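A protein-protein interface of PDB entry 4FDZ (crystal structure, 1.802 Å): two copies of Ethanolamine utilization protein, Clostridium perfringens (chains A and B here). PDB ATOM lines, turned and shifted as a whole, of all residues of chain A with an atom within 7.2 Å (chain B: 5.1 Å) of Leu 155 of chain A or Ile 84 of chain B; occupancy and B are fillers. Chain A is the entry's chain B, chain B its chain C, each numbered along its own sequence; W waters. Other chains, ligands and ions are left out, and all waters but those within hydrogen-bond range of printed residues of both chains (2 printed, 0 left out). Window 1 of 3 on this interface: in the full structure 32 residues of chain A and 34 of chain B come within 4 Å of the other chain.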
ATOM      1  N   ALA A 152      -3.008 -16.472 -33.606  1.00  0.00           N
ATOM      2  CA  ALA A 152      -3.316 -17.492 -32.604  1.00  0.00           C
ATOM      3  C   ALA A 152      -4.814 -17.792 -32.631  1.00  0.00           C
ATOM      4  O   ALA A 152      -5.565 -17.118 -33.335  1.00  0.00           O
ATOM      5  CB  ALA A 152      -2.882 -17.035 -31.212  1.00  0.00           C
ATOM      6  N   PRO A 153      -5.262 -18.809 -31.870  1.00  0.00           N
ATOM      7  CA  PRO A 153      -6.709 -19.046 -31.852  1.00  0.00           C
ATOM      8  C   PRO A 153      -7.416 -17.847 -31.208  1.00  0.00           C
ATOM      9  O   PRO A 153      -6.722 -17.005 -30.646  1.00  0.00           O
ATOM     10  CB  PRO A 153      -6.846 -20.331 -31.035  1.00  0.00           C
ATOM     11  CG  PRO A 153      -5.518 -21.028 -31.225  1.00  0.00           C
ATOM     12  CD  PRO A 153      -4.520 -19.905 -31.225  1.00  0.00           C
ATOM     13  N   PRO A 154      -8.746 -17.746 -31.341  1.00  0.00           N
ATOM     14  CA  PRO A 154      -9.455 -16.482 -31.064  1.00  0.00           C
ATOM     15  C   PRO A 154      -9.163 -15.796 -29.730  1.00  0.00           C
ATOM     16  O   PRO A 154      -8.716 -14.644 -29.726  1.00  0.00           O
ATOM     17  CB  PRO A 154     -10.928 -16.879 -31.207  1.00  0.00           C
ATOM     18  CG  PRO A 154     -10.865 -17.933 -32.309  1.00  0.00           C
ATOM     19  CD  PRO A 154      -9.638 -18.741 -31.964  1.00  0.00           C
ATOM     20  N   LEU A 155      -9.386 -16.469 -28.614  1.00  0.00           N
ATOM     21  CA  LEU A 155      -9.197 -15.811 -27.334  1.00  0.00           C
ATOM     22  C   LEU A 155      -7.730 -15.539 -27.069  1.00  0.00           C
ATOM     23  O   LEU A 155      -7.364 -14.450 -26.611  1.00  0.00           O
ATOM     24  CB  LEU A 155      -9.809 -16.637 -26.207  1.00  0.00           C
ATOM     25  CG  LEU A 155      -9.740 -15.974 -24.830  1.00  0.00           C
ATOM     26  CD1 LEU A 155     -10.975 -16.282 -24.012  1.00  0.00           C
ATOM     27  CD2 LEU A 155      -8.496 -16.432 -24.077  1.00  0.00           C
ATOM     28  N   GLU A 156      -6.883 -16.526 -27.349  1.00  0.00           N
ATOM     29  CA  GLU A 156      -5.450 -16.356 -27.155  1.00  0.00           C
ATOM     30  C   GLU A 156      -4.947 -15.142 -27.927  1.00  0.00           C
ATOM     31  O   GLU A 156      -4.101 -14.395 -27.437  1.00  0.00           O
ATOM     32  CB  GLU A 156      -4.697 -17.601 -27.627  1.00  0.00           C
ATOM     33  CG  GLU A 156      -4.995 -18.850 -26.819  1.00  0.00           C
ATOM     34  CD  GLU A 156      -6.050 -19.727 -27.474  1.00  0.00           C
ATOM     35  OE1 GLU A 156      -7.118 -19.192 -27.835  1.00  0.00           O
ATOM     36  OE2 GLU A 156      -5.788 -20.940 -27.679  1.00  0.00           O
ATOM     37  N   ALA A 157      -5.443 -14.967 -29.148  1.00  0.00           N
ATOM     38  CA  ALA A 157      -4.981 -13.873 -29.990  1.00  0.00           C
ATOM     39  C   ALA A 157      -5.367 -12.510 -29.408  1.00  0.00           C
ATOM     40  O   ALA A 157      -4.567 -11.571 -29.415  1.00  0.00           O
ATOM     41  CB  ALA A 157      -5.545 -14.020 -31.412  1.00  0.00           C
ATOM     42  N   MET A 158      -6.597 -12.381 -28.931  1.00  0.00           N
ATOM     43  CA  MET A 158      -7.046 -11.103 -28.404  1.00  0.00           C
ATOM     44  C   MET A 158      -6.239 -10.754 -27.147  1.00  0.00           C
ATOM     45  O   MET A 158      -5.732  -9.635 -27.017  1.00  0.00           O
ATOM     46  CB  MET A 158      -8.549 -11.132 -28.128  1.00  0.00           C
ATOM     47  CG  MET A 158      -9.394 -11.378 -29.375  1.00  0.00           C
ATOM     48  SD  MET A 158      -9.127 -10.174 -30.705  1.00  0.00           S
ATOM     49  CE  MET A 158      -9.796  -8.700 -29.936  1.00  0.00           C
ATOM     50  N   TYR A 159      -6.097 -11.720 -26.247  1.00  0.00           N
ATOM     51  CA  TYR A 159      -5.328 -11.544 -25.011  1.00  0.00           C
ATOM     52  C   TYR A 159      -3.855 -11.223 -25.310  1.00  0.00           C
ATOM     53  O   TYR A 159      -3.271 -10.308 -24.717  1.00  0.00           O
ATOM     54  CB  TYR A 159      -5.438 -12.830 -24.198  1.00  0.00           C
ATOM     55  CG  TYR A 159      -4.803 -12.808 -22.821  1.00  0.00           C
ATOM     56  CD1 TYR A 159      -5.490 -12.308 -21.720  1.00  0.00           C
ATOM     57  CD2 TYR A 159      -3.529 -13.313 -22.622  1.00  0.00           C
ATOM     58  CE1 TYR A 159      -4.908 -12.308 -20.454  1.00  0.00           C
ATOM     59  CE2 TYR A 159      -2.949 -13.314 -21.370  1.00  0.00           C
ATOM     60  CZ  TYR A 159      -3.637 -12.822 -20.299  1.00  0.00           C
ATOM     61  OH  TYR A 159      -3.018 -12.841 -19.072  1.00  0.00           O
ATOM     62  N   ALA A 160      -3.267 -11.971 -26.245  1.00  0.00           N
ATOM     63  CA  ALA A 160      -1.845 -11.833 -26.553  1.00  0.00           C
ATOM     64  C   ALA A 160      -1.540 -10.582 -27.378  1.00  0.00           C
ATOM     65  O   ALA A 160      -0.454 -10.016 -27.267  1.00  0.00           O
ATOM     66  CB  ALA A 160      -1.338 -13.083 -27.273  1.00  0.00           C
ATOM     67  N   LEU A 161      -2.492 -10.139 -28.198  1.00  0.00           N
ATOM     68  CA  LEU A 161      -2.299  -8.892 -28.936  1.00  0.00           C
ATOM     69  C   LEU A 161      -2.214  -7.736 -27.957  1.00  0.00           C
ATOM     70  O   LEU A 161      -1.377  -6.839 -28.088  1.00  0.00           O
ATOM     71  CB  LEU A 161      -3.446  -8.645 -29.920  1.00  0.00           C
ATOM     72  CG  LEU A 161      -3.380  -9.402 -31.242  1.00  0.00           C
ATOM     73  CD1 LEU A 161      -4.635  -9.114 -32.036  1.00  0.00           C
ATOM     74  CD2 LEU A 161      -2.133  -9.007 -32.029  1.00  0.00           C
ATOM     75  N   ALA A 177      -9.882 -10.240 -37.463  1.00  0.00           N
ATOM     76  CA  ALA A 177     -10.937 -10.417 -36.467  1.00  0.00           C
ATOM     77  C   ALA A 177     -11.422 -11.864 -36.466  1.00  0.00           C
ATOM     78  O   ALA A 177     -11.632 -12.438 -37.528  1.00  0.00           O
ATOM     79  CB  ALA A 177     -12.083  -9.476 -36.767  1.00  0.00           C
ATOM     80  N   PRO A 178     -11.582 -12.472 -35.276  1.00  0.00           N
ATOM     81  CA  PRO A 178     -11.980 -13.886 -35.234  1.00  0.00           C
ATOM     82  C   PRO A 178     -13.447 -14.085 -35.594  1.00  0.00           C
ATOM     83  O   PRO A 178     -14.294 -13.324 -35.119  1.00  0.00           O
ATOM     84  CB  PRO A 178     -11.740 -14.282 -33.771  1.00  0.00           C
ATOM     85  CG  PRO A 178     -11.770 -12.999 -33.009  1.00  0.00           C
ATOM     86  CD  PRO A 178     -11.271 -11.937 -33.947  1.00  0.00           C
ATOM     87  N   PRO A 179     -13.748 -15.095 -36.423  1.00  0.00           N
ATOM     88  CA  PRO A 179     -12.810 -16.032 -37.049  1.00  0.00           C
ATOM     89  C   PRO A 179     -12.280 -15.576 -38.399  1.00  0.00           C
ATOM     90  O   PRO A 179     -13.035 -14.990 -39.198  1.00  0.00           O
ATOM     91  CB  PRO A 179     -13.690 -17.263 -37.300  1.00  0.00           C
ATOM     92  CG  PRO A 179     -15.028 -16.672 -37.601  1.00  0.00           C
ATOM     93  CD  PRO A 179     -15.150 -15.468 -36.698  1.00  0.00           C
ATOM     94  N   ALA A 185      -7.065 -15.842 -35.439  1.00  0.00           N
ATOM     95  CA  ALA A 185      -7.163 -14.389 -35.319  1.00  0.00           C
ATOM     96  C   ALA A 185      -5.770 -13.838 -35.062  1.00  0.00           C
ATOM     97  O   ALA A 185      -4.817 -14.596 -34.913  1.00  0.00           O
ATOM     98  CB  ALA A 185      -8.097 -14.002 -34.185  1.00  0.00           C
ATOM     99  N   VAL A 210      -1.936 -18.439 -21.596  1.00  0.00           N
ATOM    100  CA  VAL A 210      -3.345 -18.839 -21.660  1.00  0.00           C
ATOM    101  C   VAL A 210      -3.451 -20.361 -21.728  1.00  0.00           C
ATOM    102  O   VAL A 210      -4.301 -20.975 -21.082  1.00  0.00           O
ATOM    103  CB  VAL A 210      -4.083 -18.219 -22.879  1.00  0.00           C
ATOM    104  CG1 VAL A 210      -5.510 -18.726 -22.948  1.00  0.00           C
ATOM    105  CG2 VAL A 210      -4.073 -16.703 -22.786  1.00  0.00           C
ATOM    106  N   PRO A 214      -6.112 -21.752 -18.823  1.00  0.00           N
ATOM    107  CA  PRO A 214      -7.119 -21.255 -19.779  1.00  0.00           C
ATOM    108  C   PRO A 214      -8.356 -20.651 -19.134  1.00  0.00           C
ATOM    109  O   PRO A 214      -9.000 -19.803 -19.757  1.00  0.00           O
ATOM    110  CB  PRO A 214      -7.483 -22.492 -20.610  1.00  0.00           C
ATOM    111  CG  PRO A 214      -6.924 -23.676 -19.868  1.00  0.00           C
ATOM    112  CD  PRO A 214      -5.818 -23.185 -18.985  1.00  0.00           C
ATOM    113  N   SER B  12     -12.357 -21.385 -22.307  1.00  0.00           N
ATOM    114  CA  SER B  12     -11.401 -20.395 -21.841  1.00  0.00           C
ATOM    115  C   SER B  12     -12.097 -19.098 -21.429  1.00  0.00           C
ATOM    116  O   SER B  12     -13.117 -18.711 -22.024  1.00  0.00           O
ATOM    117  CB  SER B  12     -10.366 -20.126 -22.938  1.00  0.00           C
ATOM    118  OG  SER B  12      -9.307 -19.307 -22.473  1.00  0.00           O
ATOM    119  N   VAL B  13     -11.540 -18.445 -20.416  1.00  0.00           N
ATOM    120  CA  VAL B  13     -12.020 -17.155 -19.929  1.00  0.00           C
ATOM    121  C   VAL B  13     -10.835 -16.326 -19.453  1.00  0.00           C
ATOM    122  O   VAL B  13     -10.022 -16.804 -18.658  1.00  0.00           O
ATOM    123  CB  VAL B  13     -12.967 -17.321 -18.739  1.00  0.00           C
ATOM    124  CG1 VAL B  13     -13.602 -15.981 -18.364  1.00  0.00           C
ATOM    125  CG2 VAL B  13     -14.039 -18.327 -19.050  1.00  0.00           C
ATOM    126  N   LYS B  14     -10.738 -15.089 -19.921  1.00  0.00           N
ATOM    127  CA  LYS B  14      -9.658 -14.199 -19.511  1.00  0.00           C
ATOM    128  C   LYS B  14     -10.144 -12.760 -19.426  1.00  0.00           C
ATOM    129  O   LYS B  14     -11.180 -12.406 -19.998  1.00  0.00           O
ATOM    130  CB  LYS B  14      -8.492 -14.282 -20.498  1.00  0.00           C
ATOM    131  CG  LYS B  14      -7.714 -15.577 -20.437  1.00  0.00           C
ATOM    132  CD  LYS B  14      -7.014 -15.705 -19.097  1.00  0.00           C
ATOM    133  CE  LYS B  14      -6.157 -16.937 -19.015  1.00  0.00           C
ATOM    134  NZ  LYS B  14      -5.469 -17.016 -17.704  1.00  0.00           N
ATOM    135  N   LEU B  38     -13.089 -11.919 -21.904  1.00  0.00           N
ATOM    136  CA  LEU B  38     -13.065 -12.792 -23.073  1.00  0.00           C
ATOM    137  C   LEU B  38     -13.540 -14.187 -22.684  1.00  0.00           C
ATOM    138  O   LEU B  38     -13.143 -14.699 -21.632  1.00  0.00           O
ATOM    139  CB  LEU B  38     -11.634 -12.920 -23.591  1.00  0.00           C
ATOM    140  CG  LEU B  38     -10.827 -11.641 -23.808  1.00  0.00           C
ATOM    141  CD1 LEU B  38      -9.333 -11.996 -24.010  1.00  0.00           C
ATOM    142  CD2 LEU B  38     -11.352 -10.884 -25.002  1.00  0.00           C
ATOM    143  N   ILE B  39     -14.351 -14.816 -23.533  1.00  0.00           N
ATOM    144  CA  ILE B  39     -14.803 -16.182 -23.274  1.00  0.00           C
ATOM    145  C   ILE B  39     -14.971 -17.000 -24.553  1.00  0.00           C
ATOM    146  O   ILE B  39     -15.435 -16.496 -25.573  1.00  0.00           O
ATOM    147  CB  ILE B  39     -16.128 -16.197 -22.468  1.00  0.00           C
ATOM    148  CG1 ILE B  39     -16.465 -17.621 -22.011  1.00  0.00           C
ATOM    149  CG2 ILE B  39     -17.275 -15.581 -23.273  1.00  0.00           C
ATOM    150  CD1 ILE B  39     -17.615 -17.669 -20.978  1.00  0.00           C
ATOM    151  N   THR B  40     -14.580 -18.267 -24.502  1.00  0.00           N
ATOM    152  CA  THR B  40     -14.906 -19.200 -25.577  1.00  0.00           C
ATOM    153  C   THR B  40     -15.567 -20.437 -24.993  1.00  0.00           C
ATOM    154  O   THR B  40     -15.370 -20.764 -23.830  1.00  0.00           O
ATOM    155  CB  THR B  40     -13.677 -19.638 -26.374  1.00  0.00           C
ATOM    156  OG1 THR B  40     -12.817 -20.422 -25.539  1.00  0.00           O
ATOM    157  CG2 THR B  40     -12.926 -18.424 -26.914  1.00  0.00           C
ATOM    158  N   TYR B  48     -24.251 -17.055 -26.344  1.00  0.00           N
ATOM    159  CA  TYR B  48     -24.862 -15.763 -26.621  1.00  0.00           C
ATOM    160  C   TYR B  48     -25.970 -15.463 -25.619  1.00  0.00           C
ATOM    161  O   TYR B  48     -26.151 -14.317 -25.192  1.00  0.00           O
ATOM    162  CB  TYR B  48     -25.433 -15.745 -28.039  1.00  0.00           C
ATOM    163  CG  TYR B  48     -24.386 -15.892 -29.125  1.00  0.00           C
ATOM    164  CD1 TYR B  48     -23.143 -15.263 -29.014  1.00  0.00           C
ATOM    165  CD2 TYR B  48     -24.633 -16.655 -30.254  1.00  0.00           C
ATOM    166  CE1 TYR B  48     -22.181 -15.394 -30.000  1.00  0.00           C
ATOM    167  CE2 TYR B  48     -23.673 -16.788 -31.254  1.00  0.00           C
ATOM    168  CZ  TYR B  48     -22.447 -16.145 -31.118  1.00  0.00           C
ATOM    169  OH  TYR B  48     -21.481 -16.266 -32.101  1.00  0.00           O
ATOM    170  N   TYR B  64     -18.507  -7.991 -28.731  1.00  0.00           N
ATOM    171  CA  TYR B  64     -18.040  -8.913 -29.764  1.00  0.00           C
ATOM    172  C   TYR B  64     -18.677 -10.266 -29.530  1.00  0.00           C
ATOM    173  O   TYR B  64     -18.742 -10.745 -28.395  1.00  0.00           O
ATOM    174  CB  TYR B  64     -16.511  -9.035 -29.731  1.00  0.00           C
ATOM    175  CG  TYR B  64     -15.911  -9.533 -31.026  1.00  0.00           C
ATOM    176  CD1 TYR B  64     -15.454  -8.639 -31.986  1.00  0.00           C
ATOM    177  CD2 TYR B  64     -15.807 -10.894 -31.295  1.00  0.00           C
ATOM    178  CE1 TYR B  64     -14.907  -9.082 -33.178  1.00  0.00           C
ATOM    179  CE2 TYR B  64     -15.269 -11.349 -32.497  1.00  0.00           C
ATOM    180  CZ  TYR B  64     -14.815 -10.431 -33.430  1.00  0.00           C
ATOM    181  OH  TYR B  64     -14.265 -10.844 -34.629  1.00  0.00           O
ATOM    182  N   ALA B  65     -19.155 -10.884 -30.605  1.00  0.00           N
ATOM    183  CA  ALA B  65     -19.844 -12.165 -30.499  1.00  0.00           C
ATOM    184  C   ALA B  65     -19.883 -12.850 -31.851  1.00  0.00           C
ATOM    185  O   ALA B  65     -20.724 -12.528 -32.690  1.00  0.00           O
ATOM    186  CB  ALA B  65     -21.257 -11.956 -29.977  1.00  0.00           C
ATOM    187  N   ARG B  66     -18.973 -13.793 -32.068  1.00  0.00           N
ATOM    188  CA  ARG B  66     -18.879 -14.481 -33.347  1.00  0.00           C
ATOM    189  C   ARG B  66     -18.723 -15.991 -33.180  1.00  0.00           C
ATOM    190  O   ARG B  66     -18.106 -16.477 -32.224  1.00  0.00           O
ATOM    191  CB  ARG B  66     -17.701 -13.946 -34.174  1.00  0.00           C
ATOM    192  CG  ARG B  66     -17.813 -12.487 -34.590  1.00  0.00           C
ATOM    193  CD  ARG B  66     -18.912 -12.248 -35.629  1.00  0.00           C
ATOM    194  NE  ARG B  66     -18.822 -13.161 -36.776  1.00  0.00           N
ATOM    195  CZ  ARG B  66     -17.933 -13.067 -37.763  1.00  0.00           C
ATOM    196  NH1 ARG B  66     -17.032 -12.092 -37.779  1.00  0.00           N
ATOM    197  NH2 ARG B  66     -17.935 -13.964 -38.744  1.00  0.00           N
ATOM    198  N   MET B  68     -17.618 -19.865 -34.932  1.00  0.00           N
ATOM    199  CA  MET B  68     -16.537 -20.434 -35.733  1.00  0.00           C
ATOM    200  C   MET B  68     -17.059 -21.312 -36.873  1.00  0.00           C
ATOM    201  O   MET B  68     -18.043 -22.045 -36.720  1.00  0.00           O
ATOM    202  CB  MET B  68     -15.615 -21.272 -34.854  1.00  0.00           C
ATOM    203  CG  MET B  68     -15.068 -20.523 -33.638  1.00  0.00           C
ATOM    204  SD  MET B  68     -13.871 -19.259 -34.112  1.00  0.00           S
ATOM    205  CE  MET B  68     -14.606 -17.770 -33.477  1.00  0.00           C
ATOM    206  N   GLU B  82     -16.570 -23.079 -30.676  1.00  0.00           N
ATOM    207  CA  GLU B  82     -17.286 -22.495 -31.799  1.00  0.00           C
ATOM    208  C   GLU B  82     -17.801 -21.094 -31.512  1.00  0.00           C
ATOM    209  O   GLU B  82     -18.652 -20.601 -32.236  1.00  0.00           O
ATOM    210  CB  GLU B  82     -18.445 -23.390 -32.259  1.00  0.00           C
ATOM    211  CG  GLU B  82     -19.566 -23.557 -31.233  1.00  0.00           C
ATOM    212  CD  GLU B  82     -20.691 -24.468 -31.719  1.00  0.00           C
ATOM    213  OE1 GLU B  82     -20.404 -25.438 -32.473  1.00  0.00           O
ATOM    214  OE2 GLU B  82     -21.860 -24.213 -31.340  1.00  0.00           O
ATOM    215  N   VAL B  83     -17.281 -20.437 -30.479  1.00  0.00           N
ATOM    216  CA  VAL B  83     -17.731 -19.075 -30.197  1.00  0.00           C
ATOM    217  C   VAL B  83     -16.681 -18.284 -29.434  1.00  0.00           C
ATOM    218  O   VAL B  83     -15.958 -18.836 -28.592  1.00  0.00           O
ATOM    219  CB  VAL B  83     -19.078 -19.081 -29.420  1.00  0.00           C
ATOM    220  CG1 VAL B  83     -18.920 -19.733 -28.074  1.00  0.00           C
ATOM    221  CG2 VAL B  83     -19.639 -17.667 -29.278  1.00  0.00           C
ATOM    222  N   ILE B  84     -16.579 -16.997 -29.752  1.00  0.00           N
ATOM    223  CA  ILE B  84     -15.847 -16.067 -28.904  1.00  0.00           C
ATOM    224  C   ILE B  84     -16.781 -14.922 -28.569  1.00  0.00           C
ATOM    225  O   ILE B  84     -17.455 -14.384 -29.454  1.00  0.00           O
ATOM    226  CB  ILE B  84     -14.546 -15.529 -29.545  1.00  0.00           C
ATOM    227  CG1 ILE B  84     -13.876 -14.550 -28.570  1.00  0.00           C
ATOM    228  CG2 ILE B  84     -14.817 -14.897 -30.916  1.00  0.00           C
ATOM    229  CD1 ILE B  84     -12.440 -14.224 -28.859  1.00  0.00           C
ATOM    230  N   GLY B  85     -16.865 -14.617 -27.279  1.00  0.00           N
ATOM    231  CA  GLY B  85     -17.624 -13.481 -26.795  1.00  0.00           C
ATOM    232  C   GLY B  85     -16.720 -12.504 -26.054  1.00  0.00           C
ATOM    233  O   GLY B  85     -15.761 -12.904 -25.393  1.00  0.00           O
ATOM    234  N   ILE B  86     -17.017 -11.215 -26.175  1.00  0.00           N
ATOM    235  CA  ILE B  86     -16.260 -10.204 -25.454  1.00  0.00           C
ATOM    236  C   ILE B  86     -17.202  -9.240 -24.784  1.00  0.00           C
ATOM    237  O   ILE B  86     -18.059  -8.630 -25.432  1.00  0.00           O
ATOM    238  CB  ILE B  86     -15.301  -9.419 -26.365  1.00  0.00           C
ATOM    239  CG1 ILE B  86     -14.354 -10.383 -27.077  1.00  0.00           C
ATOM    240  CG2 ILE B  86     -14.516  -8.384 -25.542  1.00  0.00           C
ATOM    241  CD1 ILE B  86     -13.377  -9.692 -28.052  1.00  0.00           C
HETATM  242  O   HOH W   1     -14.390 -12.474 -39.069  1.00  0.00           O
HETATM  243  O   HOH W   2      -2.923 -15.961 -18.760  1.00  0.00           O
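No position is printed for both chains.
Water W1 lies within hydrogen-bond range of O of Pro 179 of chain A (2.9 Å), NH1 of Arg 66 of chain B (3.0 Å) and O of Ala 177 of chain A (3.2 Å).
Water W2 bridges the side-chain amino group (NZ) of Lys 14 of chain B (3.0 Å) and the side-chain hydroxyl (OH) of Tyr 159 of chain A (3.1 Å).
The backbone carbonyl oxygen (O) of Pro 178 of chain A sits at hydrogen-bond distance from the side-chain hydroxyl (OH) of Tyr 64 of chain B (2.5 Å).
OG of Ser 12 of chain B is in hydrogen-bond range of O of Pro 214 of chain A, at 2.8 Å.
The backbone carbonyl oxygen (O) of Pro 214 of chain A is in hydrogen-bond range of the backbone NH (N) of Val 13 of chain B, at 3.0 Å.
Pro 154 of chain A touches Met 68 of chain B (CG to SD, 3.7 Å).
Ile 84 of chain B touches Pro 154 of chain A (CD1 to C, 3.7 Å).
Leu 155 of chain A touches Lys 14 of chain B.
N of Ile 39 of chain B touches CD1 of Leu 155 of chain A (3.7 Å).
Thr 40 of chain B touches Leu 155 of chain A (CG2 to CB, 3.7 Å).
Leu 155 of chain A touches Ile 84 of chain B (N to CD1, 3.8 Å).
Tyr 159 of chain A touches Leu 38 of chain B.
Arg 66 of chain B touches Pro 179 of chain A (NH2 to CD, 3.8 Å).
Met 68 of chain B touches Pro 179 of chain A (SD to CB, 3.8 Å).
Val 210 of chain A touches Ser 12 of chain B (CG1 to OG, 3.9 Å).
Hydrophobic or aromatic side chains of chain B within 4 Å of the printed part of chain A: Leu 38, Tyr 64, Met 68 and Ile 84.
Printed residues of chain A that touch a printed residue of chain B: Pro 154, Leu 155, Tyr 159, Ala 177, Pro 178, Pro 179, Val 210 and Pro 214.
Hydrophobic or aromatic side chains of chain A within 4 Å of the printed part of chain B: Pro 154, Leu 155, Tyr 159, Ala 177, Pro 178, Pro 179 and Val 210.
Printed residues of chain B within 4 Å of Leu 155 of chain A: Ser 12 (3.4 Å), Lys 14 (3.8 Å), Leu 38 (3.5 Å), Ile 39 (3.7 Å), Thr 40 (3.7 Å) and Ile 84 (3.8 Å).
Of the printed residues of chain A, Leu 38 of chain B touches Leu 155 (3.5 Å) and Tyr 159 (3.9 Å).
Of the printed residues of chain A, Tyr 64 of chain B touches Ala 177 (3.3 Å) and Pro 178 (2.5 Å).
Printed residues of chain A within 4 Å of Ile 84 of chain B: Pro 154 (3.7 Å) and Leu 155 (3.8 Å).
The nearest printed residue of chain B that does not touch Leu 155 of chain A is Val 13 of chain B (4.2 Å).
The nearest printed residue of chain A that does not touch Ile 84 of chain B is Pro 178 of chain A (4.2 Å).
The nearest printed residue of chain A that does not touch Thr 40 of chain B is Pro 154 of chain A (5.0 Å).
The backbone carbonyl oxygen (O) of Lys 14 of chain B lies within hydrogen-bond range of the backbone NH (N) of Leu 38 of chain B (2.7 Å).
The backbone NH (N) of Gly 85 of chain B lies within hydrogen-bond range of the backbone carbonyl oxygen (O) of Ile 39 of chain B (2.9 Å).
OH of Tyr 48 of chain B lies close to O of Arg 66 of chain B (3.4 Å).
The backbone NH of Ile 86 of chain B sits at hydrogen-bond distance from the backbone carbonyl oxygen of Tyr 64 of chain B, at 2.9 Å.
The backbone NH of Ile 84 of chain B lies within hydrogen-bond range of the backbone carbonyl oxygen of Arg 66 of chain B.
The backbone NH of Met 68 of chain B is in hydrogen-bond range of the backbone carbonyl oxygen of Glu 82 of chain B, at 3.0 Å.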
